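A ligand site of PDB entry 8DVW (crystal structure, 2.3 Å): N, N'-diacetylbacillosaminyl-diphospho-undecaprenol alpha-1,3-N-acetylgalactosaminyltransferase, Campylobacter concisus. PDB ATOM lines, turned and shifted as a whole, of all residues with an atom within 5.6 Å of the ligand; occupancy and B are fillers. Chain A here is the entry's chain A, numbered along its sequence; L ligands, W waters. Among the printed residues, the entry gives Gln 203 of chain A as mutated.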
ATOM      1  N   MET A  12      -1.323 -22.811   5.986  1.00  0.00           N
ATOM      2  CA  MET A  12      -1.048 -24.073   5.311  1.00  0.00           C
ATOM      3  C   MET A  12      -0.071 -23.890   4.157  1.00  0.00           C
ATOM      4  O   MET A  12       0.758 -24.774   3.927  1.00  0.00           O
ATOM      5  CB  MET A  12      -2.346 -24.714   4.806  1.00  0.00           C
ATOM      6  CG  MET A  12      -3.054 -23.975   3.692  1.00  0.00           C
ATOM      7  SD  MET A  12      -2.354 -24.262   2.040  1.00  0.00           S
ATOM      8  CE  MET A  12      -2.634 -26.025   1.814  1.00  0.00           C
ATOM      9  N   SER A  13      -0.139 -22.750   3.454  1.00  0.00           N
ATOM     10  CA  SER A  13       0.803 -22.503   2.380  1.00  0.00           C
ATOM     11  C   SER A  13       2.221 -22.368   2.922  1.00  0.00           C
ATOM     12  O   SER A  13       3.172 -22.852   2.299  1.00  0.00           O
ATOM     13  CB  SER A  13       0.410 -21.236   1.603  1.00  0.00           C
ATOM     14  OG  SER A  13      -0.892 -21.384   1.065  1.00  0.00           O
ATOM     15  N   PHE A  16       3.238 -26.167   4.218  1.00  0.00           N
ATOM     16  CA  PHE A  16       3.363 -27.219   3.222  1.00  0.00           C
ATOM     17  C   PHE A  16       4.174 -26.801   1.997  1.00  0.00           C
ATOM     18  O   PHE A  16       4.870 -27.642   1.404  1.00  0.00           O
ATOM     19  CB  PHE A  16       1.986 -27.684   2.718  1.00  0.00           C
ATOM     20  CG  PHE A  16       1.166 -28.408   3.742  1.00  0.00           C
ATOM     21  CD1 PHE A  16       1.555 -29.642   4.209  1.00  0.00           C
ATOM     22  CD2 PHE A  16      -0.023 -27.860   4.210  1.00  0.00           C
ATOM     23  CE1 PHE A  16       0.809 -30.321   5.164  1.00  0.00           C
ATOM     24  CE2 PHE A  16      -0.796 -28.532   5.154  1.00  0.00           C
ATOM     25  CZ  PHE A  16      -0.380 -29.773   5.633  1.00  0.00           C
ATOM     26  N   PHE A  17       4.116 -25.536   1.607  1.00  0.00           N
ATOM     27  CA  PHE A  17       4.692 -25.088   0.346  1.00  0.00           C
ATOM     28  C   PHE A  17       5.968 -24.281   0.517  1.00  0.00           C
ATOM     29  O   PHE A  17       6.987 -24.621  -0.100  1.00  0.00           O
ATOM     30  CB  PHE A  17       3.646 -24.279  -0.437  1.00  0.00           C
ATOM     31  CG  PHE A  17       2.329 -24.999  -0.634  1.00  0.00           C
ATOM     32  CD1 PHE A  17       2.291 -26.360  -0.796  1.00  0.00           C
ATOM     33  CD2 PHE A  17       1.137 -24.299  -0.628  1.00  0.00           C
ATOM     34  CE1 PHE A  17       1.082 -27.024  -0.961  1.00  0.00           C
ATOM     35  CE2 PHE A  17      -0.075 -24.955  -0.804  1.00  0.00           C
ATOM     36  CZ  PHE A  17      -0.095 -26.310  -0.977  1.00  0.00           C
ATOM     37  N   ARG A  18       5.951 -23.249   1.364  1.00  0.00           N
ATOM     38  CA  ARG A  18       7.144 -22.409   1.499  1.00  0.00           C
ATOM     39  C   ARG A  18       8.225 -23.092   2.332  1.00  0.00           C
ATOM     40  O   ARG A  18       9.419 -22.791   2.183  1.00  0.00           O
ATOM     41  CB  ARG A  18       6.787 -21.068   2.140  1.00  0.00           C
ATOM     42  CG  ARG A  18       5.677 -20.290   1.484  1.00  0.00           C
ATOM     43  CD  ARG A  18       6.109 -19.733   0.142  1.00  0.00           C
ATOM     44  NE  ARG A  18       5.871 -20.698  -0.931  1.00  0.00           N
ATOM     45  CZ  ARG A  18       4.675 -21.000  -1.422  1.00  0.00           C
ATOM     46  NH1 ARG A  18       3.571 -20.447  -0.954  1.00  0.00           N
ATOM     47  NH2 ARG A  18       4.573 -21.867  -2.420  1.00  0.00           N
ATOM     48  N   GLU A 113       0.577 -19.434  -7.645  1.00  0.00           N
ATOM     49  CA  GLU A 113       0.439 -20.894  -7.669  1.00  0.00           C
ATOM     50  C   GLU A 113      -1.043 -21.218  -7.843  1.00  0.00           C
ATOM     51  O   GLU A 113      -1.703 -21.755  -6.942  1.00  0.00           O
ATOM     52  CB  GLU A 113       1.012 -21.527  -6.411  1.00  0.00           C
ATOM     53  CG  GLU A 113       0.452 -21.022  -5.100  1.00  0.00           C
ATOM     54  CD  GLU A 113       1.345 -21.375  -3.919  1.00  0.00           C
ATOM     55  OE1 GLU A 113       2.218 -22.272  -4.086  1.00  0.00           O
ATOM     56  OE2 GLU A 113       1.199 -20.751  -2.830  1.00  0.00           O
ATOM     57  N   GLY A 114      -1.578 -20.874  -9.000  1.00  0.00           N
ATOM     58  CA  GLY A 114      -2.986 -21.042  -9.312  1.00  0.00           C
ATOM     59  C   GLY A 114      -3.665 -19.692  -9.425  1.00  0.00           C
ATOM     60  O   GLY A 114      -3.362 -18.754  -8.682  1.00  0.00           O
ATOM     61  N   LEU A 115      -4.591 -19.595 -10.390  1.00  0.00           N
ATOM     62  CA  LEU A 115      -5.336 -18.356 -10.585  1.00  0.00           C
ATOM     63  C   LEU A 115      -6.605 -18.283  -9.751  1.00  0.00           C
ATOM     64  O   LEU A 115      -7.109 -17.191  -9.505  1.00  0.00           O
ATOM     65  CB  LEU A 115      -5.673 -18.189 -12.067  1.00  0.00           C
ATOM     66  CG  LEU A 115      -4.485 -18.027 -13.002  1.00  0.00           C
ATOM     67  CD1 LEU A 115      -4.960 -17.611 -14.415  1.00  0.00           C
ATOM     68  CD2 LEU A 115      -3.473 -17.017 -12.502  1.00  0.00           C
ATOM     69  N   GLY A 116      -7.129 -19.417  -9.305  1.00  0.00           N
ATOM     70  CA  GLY A 116      -8.223 -19.420  -8.345  1.00  0.00           C
ATOM     71  C   GLY A 116      -9.602 -19.383  -8.967  1.00  0.00           C
ATOM     72  O   GLY A 116      -9.786 -19.390 -10.184  1.00  0.00           O
ATOM     73  N   VAL A 150       4.625 -21.298 -10.442  1.00  0.00           N
ATOM     74  CA  VAL A 150       4.813 -22.739 -10.255  1.00  0.00           C
ATOM     75  C   VAL A 150       4.385 -23.549 -11.467  1.00  0.00           C
ATOM     76  O   VAL A 150       4.687 -24.746 -11.524  1.00  0.00           O
ATOM     77  CB  VAL A 150       4.053 -23.219  -9.009  1.00  0.00           C
ATOM     78  CG1 VAL A 150       4.386 -22.324  -7.822  1.00  0.00           C
ATOM     79  CG2 VAL A 150       2.569 -23.234  -9.266  1.00  0.00           C
ATOM     80  N   VAL A 175       6.245 -26.315  -6.408  1.00  0.00           N
ATOM     81  CA  VAL A 175       6.905 -25.898  -5.178  1.00  0.00           C
ATOM     82  C   VAL A 175       7.781 -26.999  -4.599  1.00  0.00           C
ATOM     83  O   VAL A 175       8.395 -26.800  -3.545  1.00  0.00           O
ATOM     84  CB  VAL A 175       5.858 -25.453  -4.142  1.00  0.00           C
ATOM     85  CG1 VAL A 175       5.029 -24.303  -4.689  1.00  0.00           C
ATOM     86  CG2 VAL A 175       4.962 -26.625  -3.762  1.00  0.00           C
ATOM     87  N   PHE A 182       8.452 -38.675   1.225  1.00  0.00           N
ATOM     88  CA  PHE A 182       7.469 -39.385   0.389  1.00  0.00           C
ATOM     89  C   PHE A 182       8.186 -40.454  -0.419  1.00  0.00           C
ATOM     90  O   PHE A 182       8.427 -40.330  -1.626  1.00  0.00           O
ATOM     91  CB  PHE A 182       6.731 -38.398  -0.504  1.00  0.00           C
ATOM     92  CG  PHE A 182       5.678 -37.600   0.206  1.00  0.00           C
ATOM     93  CD1 PHE A 182       6.000 -36.424   0.858  1.00  0.00           C
ATOM     94  CD2 PHE A 182       4.356 -38.030   0.213  1.00  0.00           C
ATOM     95  CE1 PHE A 182       5.026 -35.688   1.519  1.00  0.00           C
ATOM     96  CE2 PHE A 182       3.378 -37.285   0.873  1.00  0.00           C
ATOM     97  CZ  PHE A 182       3.717 -36.123   1.527  1.00  0.00           C
ATOM     98  N   ILE A 201      -7.190 -36.226  -2.146  1.00  0.00           N
ATOM     99  CA  ILE A 201      -6.717 -35.345  -1.088  1.00  0.00           C
ATOM    100  C   ILE A 201      -6.992 -33.922  -1.536  1.00  0.00           C
ATOM    101  O   ILE A 201      -6.419 -33.451  -2.528  1.00  0.00           O
ATOM    102  CB  ILE A 201      -5.224 -35.542  -0.794  1.00  0.00           C
ATOM    103  CG1 ILE A 201      -4.926 -36.967  -0.355  1.00  0.00           C
ATOM    104  CG2 ILE A 201      -4.774 -34.536   0.273  1.00  0.00           C
ATOM    105  CD1 ILE A 201      -3.466 -37.323  -0.439  1.00  0.00           C
ATOM    106  N   ALA A 202      -7.852 -33.231  -0.796  1.00  0.00           N
ATOM    107  CA  ALA A 202      -8.148 -31.847  -1.157  1.00  0.00           C
ATOM    108  C   ALA A 202      -8.996 -31.224  -0.070  1.00  0.00           C
ATOM    109  O   ALA A 202      -9.780 -31.916   0.593  1.00  0.00           O
ATOM    110  CB  ALA A 202      -8.891 -31.754  -2.495  1.00  0.00           C
ATOM    111  N   GLN A 203      -8.861 -29.906   0.099  1.00  0.00           N
ATOM    112  CA  GLN A 203      -9.870 -29.154   0.818  1.00  0.00           C
ATOM    113  C   GLN A 203     -11.169 -29.276   0.032  1.00  0.00           C
ATOM    114  O   GLN A 203     -11.146 -29.257  -1.199  1.00  0.00           O
ATOM    115  CB  GLN A 203      -9.449 -27.717   0.979  1.00  0.00           C
ATOM    116  N   LYS A 208     -12.697 -27.983  -6.366  1.00  0.00           N
ATOM    117  CA  LYS A 208     -11.729 -29.069  -6.399  1.00  0.00           C
ATOM    118  C   LYS A 208     -12.292 -30.341  -7.025  1.00  0.00           C
ATOM    119  O   LYS A 208     -11.552 -31.327  -7.157  1.00  0.00           O
ATOM    120  CB  LYS A 208     -11.254 -29.385  -4.983  1.00  0.00           C
ATOM    121  CG  LYS A 208     -10.152 -28.453  -4.468  1.00  0.00           C
ATOM    122  CD  LYS A 208      -8.806 -28.788  -5.095  1.00  0.00           C
ATOM    123  CE  LYS A 208      -7.677 -28.052  -4.364  1.00  0.00           C
ATOM    124  NZ  LYS A 208      -6.306 -28.515  -4.826  1.00  0.00           N
ATOM    125  N   VAL A 231      -9.740 -37.287   1.719  1.00  0.00           N
ATOM    126  CA  VAL A 231      -8.957 -36.725   2.813  1.00  0.00           C
ATOM    127  C   VAL A 231      -8.999 -35.211   2.654  1.00  0.00           C
ATOM    128  O   VAL A 231      -8.629 -34.690   1.592  1.00  0.00           O
ATOM    129  CB  VAL A 231      -7.511 -37.231   2.804  1.00  0.00           C
ATOM    130  CG1 VAL A 231      -6.666 -36.458   3.791  1.00  0.00           C
ATOM    131  CG2 VAL A 231      -7.488 -38.727   3.112  1.00  0.00           C
ATOM    132  N   GLY A 232      -9.433 -34.540   3.693  1.00  0.00           N
ATOM    133  CA  GLY A 232      -9.515 -33.085   3.687  1.00  0.00           C
ATOM    134  C   GLY A 232     -10.666 -32.608   4.543  1.00  0.00           C
ATOM    135  O   GLY A 232     -11.469 -33.379   5.058  1.00  0.00           O
ATOM    136  N   GLU A 233     -10.735 -31.279   4.680  1.00  0.00           N
ATOM    137  CA  GLU A 233     -11.680 -30.643   5.581  1.00  0.00           C
ATOM    138  C   GLU A 233     -12.811 -29.983   4.813  1.00  0.00           C
ATOM    139  O   GLU A 233     -12.587 -29.408   3.742  1.00  0.00           O
ATOM    140  CB  GLU A 233     -10.993 -29.585   6.447  1.00  0.00           C
ATOM    141  CG  GLU A 233     -10.440 -30.117   7.759  1.00  0.00           C
ATOM    142  CD  GLU A 233      -9.761 -29.047   8.583  1.00  0.00           C
ATOM    143  OE1 GLU A 233     -10.101 -27.851   8.416  1.00  0.00           O
ATOM    144  OE2 GLU A 233      -8.892 -29.406   9.409  1.00  0.00           O
ATOM    145  N   GLY A 256     -11.515 -36.972   6.892  1.00  0.00           N
ATOM    146  CA  GLY A 256     -11.221 -35.638   7.375  1.00  0.00           C
ATOM    147  C   GLY A 256      -9.765 -35.274   7.146  1.00  0.00           C
ATOM    148  O   GLY A 256      -9.107 -35.787   6.233  1.00  0.00           O
ATOM    149  N   ALA A 257      -9.253 -34.371   7.967  1.00  0.00           N
ATOM    150  CA  ALA A 257      -7.867 -33.947   7.890  1.00  0.00           C
ATOM    151  C   ALA A 257      -6.941 -35.016   8.453  1.00  0.00           C
ATOM    152  O   ALA A 257      -7.271 -35.713   9.424  1.00  0.00           O
ATOM    153  CB  ALA A 257      -7.672 -32.641   8.661  1.00  0.00           C
ATOM    154  N   ARG A 258      -5.770 -35.131   7.829  1.00  0.00           N
ATOM    155  CA  ARG A 258      -4.805 -36.175   8.175  1.00  0.00           C
ATOM    156  C   ARG A 258      -3.387 -35.635   8.038  1.00  0.00           C
ATOM    157  O   ARG A 258      -3.123 -34.739   7.235  1.00  0.00           O
ATOM    158  CB  ARG A 258      -4.987 -37.409   7.270  1.00  0.00           C
ATOM    159  CG  ARG A 258      -6.376 -38.049   7.333  1.00  0.00           C
ATOM    160  CD  ARG A 258      -6.567 -38.863   8.609  1.00  0.00           C
ATOM    161  NE  ARG A 258      -5.673 -40.016   8.648  1.00  0.00           N
ATOM    162  CZ  ARG A 258      -6.065 -41.270   8.822  1.00  0.00           C
ATOM    163  NH1 ARG A 258      -7.340 -41.573   9.051  1.00  0.00           N
ATOM    164  NH2 ARG A 258      -5.169 -42.247   8.780  1.00  0.00           N
ATOM    165  N   ASN A 259      -2.476 -36.191   8.837  1.00  0.00           N
ATOM    166  CA  ASN A 259      -1.067 -35.874   8.718  1.00  0.00           C
ATOM    167  C   ASN A 259      -0.221 -37.016   8.177  1.00  0.00           C
ATOM    168  O   ASN A 259       0.974 -36.825   7.967  1.00  0.00           O
ATOM    169  CB  ASN A 259      -0.495 -35.483  10.094  1.00  0.00           C
ATOM    170  CG  ASN A 259      -1.543 -34.883  11.001  1.00  0.00           C
ATOM    171  OD1 ASN A 259      -2.285 -33.978  10.609  1.00  0.00           O
ATOM    172  ND2 ASN A 259      -1.615 -35.407  12.217  1.00  0.00           N
ATOM    173  N   ILE A 261      -0.077 -38.480   5.213  1.00  0.00           N
ATOM    174  CA  ILE A 261      -0.333 -38.556   3.784  1.00  0.00           C
ATOM    175  C   ILE A 261       0.523 -39.597   3.094  1.00  0.00           C
ATOM    176  O   ILE A 261       0.008 -40.348   2.257  1.00  0.00           O
ATOM    177  CB  ILE A 261      -0.222 -37.166   3.150  1.00  0.00           C
ATOM    178  CG1 ILE A 261      -1.164 -36.160   3.805  1.00  0.00           C
ATOM    179  CG2 ILE A 261      -0.454 -37.213   1.635  1.00  0.00           C
ATOM    180  CD1 ILE A 261      -2.636 -36.546   3.692  1.00  0.00           C
ATOM    181  N   SER A 275      -9.964 -31.492 -10.206  1.00  0.00           N
ATOM    182  CA  SER A 275     -10.063 -30.070  -9.903  1.00  0.00           C
ATOM    183  C   SER A 275     -10.614 -29.306 -11.102  1.00  0.00           C
ATOM    184  O   SER A 275     -10.496 -29.729 -12.246  1.00  0.00           O
ATOM    185  CB  SER A 275      -8.713 -29.491  -9.509  1.00  0.00           C
ATOM    186  OG  SER A 275      -8.837 -28.123  -9.136  1.00  0.00           O
ATOM    187  N   LYS A 277      -9.410 -26.227 -11.524  1.00  0.00           N
ATOM    188  CA  LYS A 277      -8.267 -25.404 -11.873  1.00  0.00           C
ATOM    189  C   LYS A 277      -7.222 -25.525 -10.783  1.00  0.00           C
ATOM    190  O   LYS A 277      -7.560 -25.485  -9.594  1.00  0.00           O
ATOM    191  CB  LYS A 277      -8.686 -23.937 -12.066  1.00  0.00           C
ATOM    192  CG  LYS A 277      -7.645 -23.064 -12.760  1.00  0.00           C
ATOM    193  CD  LYS A 277      -8.246 -21.712 -13.137  1.00  0.00           C
ATOM    194  CE  LYS A 277      -8.331 -21.546 -14.647  1.00  0.00           C
ATOM    195  NZ  LYS A 277      -7.029 -21.113 -15.223  1.00  0.00           N
ATOM    196  N   GLU A 278      -5.951 -25.636 -11.204  1.00  0.00           N
ATOM    197  CA  GLU A 278      -4.848 -25.790 -10.270  1.00  0.00           C
ATOM    198  C   GLU A 278      -3.671 -24.935 -10.716  1.00  0.00           C
ATOM    199  O   GLU A 278      -3.708 -24.287 -11.761  1.00  0.00           O
ATOM    200  CB  GLU A 278      -4.410 -27.261 -10.147  1.00  0.00           C
ATOM    201  CG  GLU A 278      -5.443 -28.189  -9.536  1.00  0.00           C
ATOM    202  CD  GLU A 278      -5.681 -27.907  -8.053  1.00  0.00           C
ATOM    203  OE1 GLU A 278      -4.716 -27.494  -7.339  1.00  0.00           O
ATOM    204  OE2 GLU A 278      -6.825 -28.099  -7.599  1.00  0.00           O
ATOM    205  N   GLY A 279      -2.605 -24.926  -9.901  1.00  0.00           N
ATOM    206  CA  GLY A 279      -1.340 -24.337 -10.312  1.00  0.00           C
ATOM    207  C   GLY A 279      -0.358 -25.416 -10.721  1.00  0.00           C
ATOM    208  O   GLY A 279      -0.112 -25.619 -11.902  1.00  0.00           O
ATOM    209  N   PHE A 280       0.224 -26.091  -9.740  1.00  0.00           N
ATOM    210  CA  PHE A 280       0.938 -27.350  -9.957  1.00  0.00           C
ATOM    211  C   PHE A 280       0.612 -28.214  -8.744  1.00  0.00           C
ATOM    212  O   PHE A 280       1.314 -28.170  -7.724  1.00  0.00           O
ATOM    213  CB  PHE A 280       2.437 -27.145 -10.127  1.00  0.00           C
ATOM    214  CG  PHE A 280       3.103 -28.262 -10.876  1.00  0.00           C
ATOM    215  CD1 PHE A 280       3.361 -29.474 -10.261  1.00  0.00           C
ATOM    216  CD2 PHE A 280       3.485 -28.104 -12.200  1.00  0.00           C
ATOM    217  CE1 PHE A 280       3.985 -30.511 -10.953  1.00  0.00           C
ATOM    218  CE2 PHE A 280       4.091 -29.127 -12.895  1.00  0.00           C
ATOM    219  CZ  PHE A 280       4.354 -30.322 -12.262  1.00  0.00           C
ATOM    220  N   PRO A 281      -0.459 -28.999  -8.817  1.00  0.00           N
ATOM    221  CA  PRO A 281      -1.038 -29.565  -7.586  1.00  0.00           C
ATOM    222  C   PRO A 281      -0.039 -30.418  -6.806  1.00  0.00           C
ATOM    223  O   PRO A 281       0.601 -31.321  -7.348  1.00  0.00           O
ATOM    224  CB  PRO A 281      -2.231 -30.395  -8.108  1.00  0.00           C
ATOM    225  CG  PRO A 281      -1.908 -30.684  -9.538  1.00  0.00           C
ATOM    226  CD  PRO A 281      -1.165 -29.458 -10.030  1.00  0.00           C
ATOM    227  N   ARG A 282       0.056 -30.128  -5.516  1.00  0.00           N
ATOM    228  CA  ARG A 282       1.044 -30.797  -4.676  1.00  0.00           C
ATOM    229  C   ARG A 282       0.591 -32.200  -4.295  1.00  0.00           C
ATOM    230  O   ARG A 282       1.438 -33.079  -4.100  1.00  0.00           O
ATOM    231  CB  ARG A 282       1.328 -29.979  -3.415  1.00  0.00           C
ATOM    232  CG  ARG A 282       2.790 -29.611  -3.249  1.00  0.00           C
ATOM    233  CD  ARG A 282       3.601 -30.799  -2.747  1.00  0.00           C
ATOM    234  NE  ARG A 282       3.455 -30.950  -1.301  1.00  0.00           N
ATOM    235  CZ  ARG A 282       4.134 -30.236  -0.406  1.00  0.00           C
ATOM    236  NH1 ARG A 282       5.024 -29.342  -0.769  1.00  0.00           N
ATOM    237  NH2 ARG A 282       3.911 -30.437   0.886  1.00  0.00           N
ATOM    238  N   THR A 283      -0.712 -32.435  -4.179  1.00  0.00           N
ATOM    239  CA  THR A 283      -1.181 -33.799  -3.927  1.00  0.00           C
ATOM    240  C   THR A 283      -0.821 -34.717  -5.096  1.00  0.00           C
ATOM    241  O   THR A 283      -0.521 -35.894  -4.903  1.00  0.00           O
ATOM    242  CB  THR A 283      -2.684 -33.835  -3.673  1.00  0.00           C
ATOM    243  OG1 THR A 283      -3.372 -33.266  -4.799  1.00  0.00           O
ATOM    244  CG2 THR A 283      -3.023 -33.069  -2.406  1.00  0.00           C
ATOM    245  N   GLU A 286       2.739 -35.492  -4.562  1.00  0.00           N
ATOM    246  CA  GLU A 286       2.862 -36.475  -3.490  1.00  0.00           C
ATOM    247  C   GLU A 286       2.531 -37.874  -3.992  1.00  0.00           C
ATOM    248  O   GLU A 286       3.231 -38.843  -3.660  1.00  0.00           O
ATOM    249  CB  GLU A 286       1.979 -36.054  -2.318  1.00  0.00           C
ATOM    250  CG  GLU A 286       2.445 -34.733  -1.660  1.00  0.00           C
ATOM    251  CD  GLU A 286       1.410 -34.113  -0.736  1.00  0.00           C
ATOM    252  OE1 GLU A 286       0.272 -34.628  -0.683  1.00  0.00           O
ATOM    253  OE2 GLU A 286       1.740 -33.099  -0.077  1.00  0.00           O
HETATM  254  C1  LIG L   1      -2.341 -24.529  -4.276  1.00  0.00           C
HETATM  255  C2  LIG L   1      -2.804 -24.879  -5.700  1.00  0.00           C
HETATM  256  C3  LIG L   1      -2.067 -26.152  -6.127  1.00  0.00           C
HETATM  257  C4  LIG L   1      -0.543 -26.044  -5.956  1.00  0.00           C
HETATM  258  C5  LIG L   1      -0.253 -25.534  -4.561  1.00  0.00           C
HETATM  259  C6  LIG L   1       1.213 -25.263  -4.327  1.00  0.00           C
HETATM  260  C7  LIG L   1      -5.153 -24.434  -6.405  1.00  0.00           C
HETATM  261  C8  LIG L   1      -4.605 -23.433  -7.356  1.00  0.00           C
HETATM  262  N1  LIG L   1      -4.217 -25.078  -5.661  1.00  0.00           N
HETATM  263  O1  LIG L   1      -2.554 -25.570  -3.347  1.00  0.00           O
HETATM  264  O2  LIG L   1      -2.447 -26.402  -7.456  1.00  0.00           O
HETATM  265  O3  LIG L   1      -0.055 -25.218  -6.989  1.00  0.00           O
HETATM  266  O4  LIG L   1      -0.973 -24.329  -4.315  1.00  0.00           O
HETATM  267  O5  LIG L   1       1.769 -24.705  -5.476  1.00  0.00           O
HETATM  268  O6  LIG L   1      -6.366 -24.681  -6.338  1.00  0.00           O
HETATM  269  N2  LIG L   1      -2.918 -31.975   3.220  1.00  0.00           N
HETATM  270  C9  LIG L   1      -2.706 -32.700   4.391  1.00  0.00           C
HETATM  271  N3  LIG L   1      -3.843 -33.151   5.001  1.00  0.00           N
HETATM  272  C10 LIG L   1      -5.152 -32.968   4.589  1.00  0.00           C
HETATM  273  C11 LIG L   1      -5.264 -32.202   3.391  1.00  0.00           C
HETATM  274  C12 LIG L   1      -4.180 -31.757   2.761  1.00  0.00           C
HETATM  275  O7  LIG L   1      -1.609 -32.942   4.833  1.00  0.00           O
HETATM  276  O8  LIG L   1      -6.039 -33.427   5.262  1.00  0.00           O
HETATM  277  C13 LIG L   1      -1.773 -31.463   2.488  1.00  0.00           C
HETATM  278  C14 LIG L   1      -1.476 -32.187   1.193  1.00  0.00           C
HETATM  279  O9  LIG L   1      -0.696 -33.301   1.439  1.00  0.00           O
HETATM  280  C15 LIG L   1      -0.757 -31.082   0.387  1.00  0.00           C
HETATM  281  C16 LIG L   1      -1.527 -29.853   0.843  1.00  0.00           C
HETATM  282  O10 LIG L   1      -2.066 -30.159   2.111  1.00  0.00           O
HETATM  283  O11 LIG L   1       0.576 -30.999   0.795  1.00  0.00           O
HETATM  284  C17 LIG L   1      -2.667 -29.601  -0.139  1.00  0.00           C
HETATM  285  O12 LIG L   1      -2.167 -29.281  -1.420  1.00  0.00           O
HETATM  286  P1  LIG L   1      -3.125 -28.628  -2.561  1.00  0.00           P
HETATM  287  O13 LIG L   1      -2.250 -28.420  -3.749  1.00  0.00           O
HETATM  288  O14 LIG L   1      -4.401 -29.400  -2.657  1.00  0.00           O
HETATM  289  O15 LIG L   1      -3.423 -27.226  -1.788  1.00  0.00           O
HETATM  290  P2  LIG L   1      -3.943 -25.862  -2.502  1.00  0.00           P
HETATM  291  O16 LIG L   1      -5.031 -26.166  -3.479  1.00  0.00           O
HETATM  292  O17 LIG L   1      -4.089 -24.764  -1.504  1.00  0.00           O
HETATM  293  O   HOH W   1       1.326 -33.615   3.440  1.00  0.00           O
HETATM  294  O   HOH W   2      -6.696 -25.796  -0.526  1.00  0.00           O
HETATM  295  O   HOH W   3      -6.275 -28.639  -0.939  1.00  0.00           O
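The side-chain carboxylate (OE2) of Glu 278 is in salt-bridge range of the side-chain amino group (NZ) of Lys 208 (2.9 Å). The side-chain carboxylate (OE1) of Glu 113 lies within salt-bridge range of the guanidinium group (NH2) of Arg 18, 2.9 Å away. The guanidinium group (NH1) of Arg 282 is in hydrogen-bond range of the backbone carbonyl oxygen (O) of Phe 16 (2.8 Å). N of Ala 202 sits at hydrogen-bond distance from O of Val 231 (2.9 Å). N of Gly 232 lies within hydrogen-bond range of O of Gly 256, at 2.8 Å. The side-chain hydroxyl (OG) of Ser 275 is in hydrogen-bond range of the side-chain carboxylate (OE2) of Glu 278 (2.5 Å). OG of Ser 275 sits at hydrogen-bond distance from O of Lys 277 (3.0 Å). The backbone NH (N) of Ser 275 sits close to the backbone carbonyl oxygen (O) of Lys 208 (3.4 Å).
N3 of the ligand sits at hydrogen-bond distance from O of Arg 258 (2.8 Å). The side-chain amino group (NZ) of Lys 208 lies within salt-bridge range of an oxygen (O16) of the ligand (3.0 Å). An oxygen (O5) of the ligand is in hydrogen-bond range of the side-chain carboxylate (OE1) of Glu 113, at 2.8 Å. The backbone NH (N) of Gly 279 is in hydrogen-bond range of an oxygen (O2) of the ligand (2.9 Å). The backbone NH (N) of Phe 280 is in hydrogen-bond range of an oxygen (O3) of the ligand, at 2.9 Å. The backbone NH (N) of Arg 258 lies within hydrogen-bond range of an oxygen (O8) of the ligand. OE2 of Glu 286 lies within hydrogen-bond range of O11 of the ligand, 2.6 Å away. The backbone carbonyl oxygen of Phe 280 sits close to an oxygen (O3) of the ligand (3.3 Å). The side-chain carboxylate (OE1) of Glu 278 is in hydrogen-bond range of an oxygen (O2) of the ligand (2.5 Å). NH2 of Arg 282 lies within hydrogen-bond range of O11 of the ligand (3.4 Å). The backbone NH of Arg 282 lies within hydrogen-bond range of an oxygen (O13) of the ligand (3.4 Å).
Residues that only touch the ligand: Met 12, Phe 16, Phe 17, Gly 114, Val 175, Ile 201, Val 231, Gly 232, Gly 256, Ala 257, Ile 261, Lys 277, Pro 281 and Thr 283. Hydrophobic or aromatic side chains that line the ligand: Met 12, Phe 16, Phe 17, Val 175, Ile 201, Val 231, Ala 257 and Ile 261. Within 4 Å of the ligand: Met 12, Phe 16, Phe 17, Glu 113, Gly 114, Val 175, Ile 201, Lys 208, Val 231, Gly 232, Gly 256, Ala 257, Arg 258, Ile 261, Lys 277, Glu 278, Gly 279, Phe 280, Pro 281, Arg 282, Thr 283 and Glu 286. The nearest printed residue that does not touch the ligand is Val 150 (4.001 Å).
Water W3 lies within hydrogen-bond range of O14 of the ligand (2.7 Å) and N of Gln 203 (3.1 Å).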
